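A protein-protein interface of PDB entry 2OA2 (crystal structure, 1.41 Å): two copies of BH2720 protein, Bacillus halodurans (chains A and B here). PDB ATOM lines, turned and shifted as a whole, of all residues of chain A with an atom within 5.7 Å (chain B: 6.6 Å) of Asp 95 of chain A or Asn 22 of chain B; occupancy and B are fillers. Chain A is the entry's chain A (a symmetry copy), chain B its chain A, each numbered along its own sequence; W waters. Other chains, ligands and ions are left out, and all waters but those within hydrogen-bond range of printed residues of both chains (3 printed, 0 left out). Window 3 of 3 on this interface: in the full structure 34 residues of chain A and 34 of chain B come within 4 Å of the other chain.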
ATOM      1  N   ARG A  69      32.769 -14.770  12.922  1.00  0.00           N
ATOM      2  CA  ARG A  69      31.341 -14.928  12.950  1.00  0.00           C
ATOM      3  C   ARG A  69      31.018 -16.427  12.979  1.00  0.00           C
ATOM      4  O   ARG A  69      31.463 -17.190  12.106  1.00  0.00           O
ATOM      5  CB  ARG A  69      30.694 -14.226  11.746  1.00  0.00           C
ATOM      6  CG  ARG A  69      29.236 -13.684  11.937  1.00  0.00           C
ATOM      7  CD  ARG A  69      28.186 -14.693  11.662  1.00  0.00           C
ATOM      8  NE  ARG A  69      26.860 -14.091  11.393  1.00  0.00           N
ATOM      9  CZ  ARG A  69      25.714 -14.769  11.437  1.00  0.00           C
ATOM     10  NH1 ARG A  69      25.707 -16.050  11.778  1.00  0.00           N
ATOM     11  NH2 ARG A  69      24.556 -14.168  11.149  1.00  0.00           N
ATOM     12  N   VAL A  70      30.226 -16.828  13.963  1.00  0.00           N
ATOM     13  CA  VAL A  70      29.768 -18.197  14.084  1.00  0.00           C
ATOM     14  C   VAL A  70      28.536 -18.387  13.234  1.00  0.00           C
ATOM     15  O   VAL A  70      27.532 -17.704  13.424  1.00  0.00           O
ATOM     16  CB  VAL A  70      29.433 -18.528  15.561  1.00  0.00           C
ATOM     17  CG1 VAL A  70      28.902 -19.966  15.672  1.00  0.00           C
ATOM     18  CG2 VAL A  70      30.644 -18.362  16.427  1.00  0.00           C
ATOM     19  N   GLU A  71      28.632 -19.311  12.284  1.00  0.00           N
ATOM     20  CA  GLU A  71      27.487 -19.667  11.426  1.00  0.00           C
ATOM     21  C   GLU A  71      26.754 -20.871  11.947  1.00  0.00           C
ATOM     22  O   GLU A  71      25.512 -20.985  11.714  1.00  0.00           O
ATOM     23  CB  GLU A  71      27.939 -19.881   9.983  1.00  0.00           C
ATOM     24  CG  GLU A  71      28.273 -18.559   9.251  1.00  0.00           C
ATOM     25  CD  GLU A  71      27.031 -17.753   8.890  1.00  0.00           C
ATOM     26  OE1 GLU A  71      25.889 -18.239   8.985  1.00  0.00           O
ATOM     27  OE2 GLU A  71      27.193 -16.609   8.515  1.00  0.00           O
ATOM     28  N   PHE A  93      27.254 -18.558  19.938  1.00  0.00           N
ATOM     29  CA  PHE A  93      26.317 -19.414  19.223  1.00  0.00           C
ATOM     30  C   PHE A  93      26.162 -18.929  17.826  1.00  0.00           C
ATOM     31  O   PHE A  93      26.714 -17.909  17.417  1.00  0.00           O
ATOM     32  CB  PHE A  93      24.952 -19.353  19.930  1.00  0.00           C
ATOM     33  CG  PHE A  93      25.041 -19.617  21.386  1.00  0.00           C
ATOM     34  CD1 PHE A  93      25.165 -20.920  21.872  1.00  0.00           C
ATOM     35  CD2 PHE A  93      24.990 -18.576  22.282  1.00  0.00           C
ATOM     36  CE1 PHE A  93      25.260 -21.145  23.256  1.00  0.00           C
ATOM     37  CE2 PHE A  93      25.093 -18.799  23.650  1.00  0.00           C
ATOM     38  CZ  PHE A  93      25.252 -20.079  24.125  1.00  0.00           C
ATOM     39  N   ASP A  94      25.370 -19.673  17.059  1.00  0.00           N
ATOM     40  CA  ASP A  94      24.953 -19.248  15.780  1.00  0.00           C
ATOM     41  C   ASP A  94      24.497 -17.797  15.841  1.00  0.00           C
ATOM     42  O   ASP A  94      23.791 -17.430  16.773  1.00  0.00           O
ATOM     43  CB  ASP A  94      23.765 -20.146  15.377  1.00  0.00           C
ATOM     44  CG  ASP A  94      23.883 -21.648  15.978  1.00  0.00           C
ATOM     45  OD1 ASP A  94      23.766 -21.989  17.272  1.00  0.00           O
ATOM     46  OD2 ASP A  94      24.089 -22.518  15.118  1.00  0.00           O
ATOM     47  N   ASP A  95      24.948 -16.999  14.881  1.00  0.00           N
ATOM     48  CA  ASP A  95      24.565 -15.583  14.675  1.00  0.00           C
ATOM     49  C   ASP A  95      25.515 -14.604  15.404  1.00  0.00           C
ATOM     50  O   ASP A  95      25.361 -13.398  15.295  1.00  0.00           O
ATOM     51  CB  ASP A  95      23.177 -15.223  15.114  1.00  0.00           C
ATOM     52  CG  ASP A  95      22.091 -15.939  14.297  1.00  0.00           C
ATOM     53  OD1 ASP A  95      22.399 -16.420  13.193  1.00  0.00           O
ATOM     54  OD2 ASP A  95      20.970 -16.025  14.828  1.00  0.00           O
ATOM     55  N   TYR A  96      26.425 -15.129  16.234  1.00  0.00           N
ATOM     56  CA  TYR A  96      27.299 -14.296  17.050  1.00  0.00           C
ATOM     57  C   TYR A  96      28.589 -13.934  16.330  1.00  0.00           C
ATOM     58  O   TYR A  96      29.136 -14.726  15.551  1.00  0.00           O
ATOM     59  CB  TYR A  96      27.679 -14.971  18.379  1.00  0.00           C
ATOM     60  CG  TYR A  96      26.622 -14.945  19.399  1.00  0.00           C
ATOM     61  CD1 TYR A  96      25.318 -15.350  19.120  1.00  0.00           C
ATOM     62  CD2 TYR A  96      26.930 -14.584  20.705  1.00  0.00           C
ATOM     63  CE1 TYR A  96      24.314 -15.300  20.121  1.00  0.00           C
ATOM     64  CE2 TYR A  96      25.957 -14.579  21.699  1.00  0.00           C
ATOM     65  CZ  TYR A  96      24.654 -14.918  21.387  1.00  0.00           C
ATOM     66  OH  TYR A  96      23.675 -14.908  22.425  1.00  0.00           O
ATOM     67  N   ALA A  97      29.039 -12.715  16.604  1.00  0.00           N
ATOM     68  CA  ALA A  97      30.347 -12.256  16.169  1.00  0.00           C
ATOM     69  C   ALA A  97      31.226 -12.043  17.407  1.00  0.00           C
ATOM     70  O   ALA A  97      30.748 -11.731  18.521  1.00  0.00           O
ATOM     71  CB  ALA A  97      30.232 -10.973  15.362  1.00  0.00           C
ATOM     72  N   VAL B  20      31.668  -9.649  22.236  1.00  0.00           N
ATOM     73  CA  VAL B  20      30.818 -10.650  21.611  1.00  0.00           C
ATOM     74  C   VAL B  20      29.421 -10.018  21.461  1.00  0.00           C
ATOM     75  O   VAL B  20      28.919  -9.370  22.384  1.00  0.00           O
ATOM     76  CB  VAL B  20      30.767 -11.957  22.480  1.00  0.00           C
ATOM     77  CG1 VAL B  20      29.673 -12.863  22.063  1.00  0.00           C
ATOM     78  CG2 VAL B  20      32.101 -12.649  22.450  1.00  0.00           C
ATOM     79  N   VAL B  21      28.829 -10.236  20.302  1.00  0.00           N
ATOM     80  CA  VAL B  21      27.542  -9.606  19.955  1.00  0.00           C
ATOM     81  C   VAL B  21      26.749 -10.520  19.033  1.00  0.00           C
ATOM     82  O   VAL B  21      27.345 -11.240  18.218  1.00  0.00           O
ATOM     83  CB  VAL B  21      27.815  -8.212  19.307  1.00  0.00           C
ATOM     84  CG1 VAL B  21      28.565  -8.317  18.015  1.00  0.00           C
ATOM     85  CG2 VAL B  21      26.485  -7.425  19.172  1.00  0.00           C
ATOM     86  N   ASN B  22      25.415 -10.486  19.148  1.00  0.00           N
ATOM     87  CA  ASN B  22      24.546 -11.108  18.154  1.00  0.00           C
ATOM     88  C   ASN B  22      24.437 -10.218  16.942  1.00  0.00           C
ATOM     89  O   ASN B  22      23.682  -9.267  16.931  1.00  0.00           O
ATOM     90  CB  ASN B  22      23.211 -11.457  18.756  1.00  0.00           C
ATOM     91  CG  ASN B  22      22.334 -12.206  17.788  1.00  0.00           C
ATOM     92  OD1 ASN B  22      22.477 -12.058  16.580  1.00  0.00           O
ATOM     93  ND2 ASN B  22      21.410 -13.042  18.339  1.00  0.00           N
ATOM     94  N   ILE B  23      25.334 -10.436  15.985  1.00  0.00           N
ATOM     95  CA  ILE B  23      25.455  -9.555  14.814  1.00  0.00           C
ATOM     96  C   ILE B  23      24.253  -9.646  13.890  1.00  0.00           C
ATOM     97  O   ILE B  23      23.866  -8.665  13.271  1.00  0.00           O
ATOM     98  CB  ILE B  23      26.798  -9.811  14.017  1.00  0.00           C
ATOM     99  CG1 ILE B  23      27.083  -8.659  13.045  1.00  0.00           C
ATOM    100  CG2 ILE B  23      26.786 -11.126  13.253  1.00  0.00           C
ATOM    101  CD1 ILE B  23      27.382  -7.336  13.746  1.00  0.00           C
ATOM    102  N   GLU B  24      23.661 -10.837  13.777  1.00  0.00           N
ATOM    103  CA  GLU B  24      22.458 -10.991  12.965  1.00  0.00           C
ATOM    104  C   GLU B  24      21.380 -10.051  13.490  1.00  0.00           C
ATOM    105  O   GLU B  24      20.737  -9.303  12.740  1.00  0.00           O
ATOM    106  CB  GLU B  24      21.971 -12.441  13.030  1.00  0.00           C
ATOM    107  CG  GLU B  24      20.747 -12.741  12.177  1.00  0.00           C
ATOM    108  CD  GLU B  24      19.421 -12.690  12.878  1.00  0.00           C
ATOM    109  OE1 GLU B  24      19.286 -12.254  14.054  1.00  0.00           O
ATOM    110  OE2 GLU B  24      18.413 -13.101  12.242  1.00  0.00           O
ATOM    111  N   ASP B  25      21.173 -10.084  14.795  1.00  0.00           N
ATOM    112  CA  ASP B  25      20.103  -9.313  15.417  1.00  0.00           C
ATOM    113  C   ASP B  25      20.398  -7.823  15.402  1.00  0.00           C
ATOM    114  O   ASP B  25      19.543  -7.018  15.055  1.00  0.00           O
ATOM    115  CB  ASP B  25      19.842  -9.781  16.831  1.00  0.00           C
ATOM    116  CG  ASP B  25      18.512  -9.207  17.397  1.00  0.00           C
ATOM    117  OD1 ASP B  25      17.440  -9.388  16.753  1.00  0.00           O
ATOM    118  OD2 ASP B  25      18.594  -8.553  18.424  1.00  0.00           O
ATOM    119  N   GLU B  26      21.628  -7.423  15.718  1.00  0.00           N
ATOM    120  CA  GLU B  26      21.932  -5.979  15.675  1.00  0.00           C
ATOM    121  C   GLU B  26      21.835  -5.405  14.274  1.00  0.00           C
ATOM    122  O   GLU B  26      21.365  -4.271  14.079  1.00  0.00           O
ATOM    123  CB  GLU B  26      23.276  -5.649  16.278  1.00  0.00           C
ATOM    124  CG  GLU B  26      23.368  -6.013  17.767  1.00  0.00           C
ATOM    125  CD  GLU B  26      22.369  -5.342  18.694  1.00  0.00           C
ATOM    126  OE1 GLU B  26      21.839  -4.269  18.347  1.00  0.00           O
ATOM    127  OE2 GLU B  26      22.083  -5.928  19.772  1.00  0.00           O
ATOM    128  N   THR B  27      22.274  -6.172  13.277  1.00  0.00           N
ATOM    129  CA  THR B  27      22.203  -5.705  11.903  1.00  0.00           C
ATOM    130  C   THR B  27      20.752  -5.546  11.471  1.00  0.00           C
ATOM    131  O   THR B  27      20.374  -4.563  10.825  1.00  0.00           O
ATOM    132  CB  THR B  27      22.937  -6.675  10.965  1.00  0.00           C
ATOM    133  OG1 THR B  27      24.317  -6.738  11.359  1.00  0.00           O
ATOM    134  CG2 THR B  27      22.855  -6.199   9.536  1.00  0.00           C
ATOM    135  N   GLU B  71      22.498  -9.305   5.671  1.00  0.00           N
ATOM    136  CA  GLU B  71      21.687 -10.088   6.621  1.00  0.00           C
ATOM    137  C   GLU B  71      20.245 -10.150   6.201  1.00  0.00           C
ATOM    138  O   GLU B  71      19.551 -11.163   6.525  1.00  0.00           O
ATOM    139  CB  GLU B  71      21.824  -9.532   8.036  1.00  0.00           C
ATOM    140  CG  GLU B  71      23.186  -9.866   8.688  1.00  0.00           C
ATOM    141  CD  GLU B  71      23.302 -11.328   9.102  1.00  0.00           C
ATOM    142  OE1 GLU B  71      22.312 -12.083   9.108  1.00  0.00           O
ATOM    143  OE2 GLU B  71      24.400 -11.738   9.417  1.00  0.00           O
HETATM  144  O   HOH W   1      22.486 -14.738   9.588  1.00  0.00           O
HETATM  145  O   HOH W   2      19.584 -13.881  16.078  1.00  0.00           O
HETATM  146  O   HOH W   3      21.739 -13.616  21.213  1.00  0.00           O
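Of the 8 printed residues of chain A, 4 touch a printed residue of chain B.
Hydrophobic or aromatic side chains of chain A within 4 Å of the printed part of chain B: Tyr 96 and Ala 97.
Hydrophobic or aromatic side chains of chain B that line the printed part of chain A: Val 20 and Ile 23.
Among the printed residues, Asp or Glu carboxylates within 4 Å of a Lys or Arg side-chain nitrogen of the other chain: Arg 69 of chain A with Glu 71 of chain B (3.0 Å).
Position printed for both chains: 71.
Of the printed residues of chain B, Asp 95 of chain A touches Asn 22 (3.4 Å), Ile 23 (3.0 Å) and Glu 24 (3.4 Å).
Asn 22 of chain B touches just one residue of chain A: Asp 95 (3.4 Å).
Printed residues of chain B within 4 Å of Ala 97 of chain A: Val 20 (3.3 Å), Val 21 (2.8 Å) and Ile 23 (3.9 Å).
Of the printed residues of chain A, Val 21 of chain B touches Tyr 96 and Ala 97.
Of the printed residues of chain A, Val 20 of chain B touches Tyr 96 (3.5 Å) and Ala 97 (3.3 Å).
Asp 25 of chain B touches none of the printed residues of chain A.
Thr 27 of chain B touches none of the printed residues of chain A.
The nearest printed residue of chain A that does not touch Ile 23 of chain B is Tyr 96 of chain A (4.5 Å).
Arg 69 of chain A touches Ile 23 of chain B (NE to CG2, 3.5 Å).
Glu 24 of chain B touches Arg 69 of chain A.
Tyr 96 of chain A touches Val 20 of chain B.
Tyr 96 of chain A touches Val 21 of chain B (CA to O, 3.3 Å).
Val 20 of chain B touches Ala 97 of chain A (CA to O, 3.3 Å).
CB of Ala 97 of chain A touches CB of Ile 23 of chain B, at 3.9 Å.
Water W2 lies within hydrogen-bond range of OE1 of Glu 24 of chain B, OD2 of Asp 95 of chain A and ND2 of Asn 22 of chain B.
Water W3 lies within hydrogen-bond range of the side-chain hydroxyl of Tyr 96 of chain A (2.6 Å) and the side-chain amide nitrogen of Asn 22 of chain B (2.9 Å).
Water W1 bridges NH2 of Arg 69 of chain A (2.7 Å) and OE1 of Glu 71 of chain B (2.7 Å).
The backbone carbonyl oxygen of Val 21 of chain B is in hydrogen-bond range of the backbone NH of Ala 97 of chain A.
O of Asp 95 of chain A lies close to OD1 of Asn 22 of chain B, 3.4 Å away.
The backbone NH (N) of Ile 23 of chain B is in hydrogen-bond range of the backbone carbonyl oxygen (O) of Asp 95 of chain A (3.0 Å).
N of Glu 24 of chain B sits at hydrogen-bond distance from O of Asp 95 of chain A, 3.4 Å away.
NH2 of Arg 69 of chain A lies within salt-bridge range of OE2 of Glu 71 of chain B, at 3.0 Å.
The side-chain amide oxygen of Asn 22 of chain B sits at hydrogen-bond distance from the backbone NH of Glu 24 of chain B, at 3.3 Å.
The backbone NH of Asp 25 of chain B sits at hydrogen-bond distance from the side-chain amide oxygen of Asn 22 of chain B, 3.0 Å away.
O of Ile 23 of chain B sits at hydrogen-bond distance from OG1 of Thr 27 of chain B (2.8 Å).
NH1 of Arg 69 of chain A is in salt-bridge range of OE1 of Glu 71 of chain A, at 3.6 Å.
NH1 of Arg 69 of chain A is in salt-bridge range of OD1 of Asp 95 of chain A.
N of Val 70 of chain A lies within hydrogen-bond range of O of Tyr 96 of chain A.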
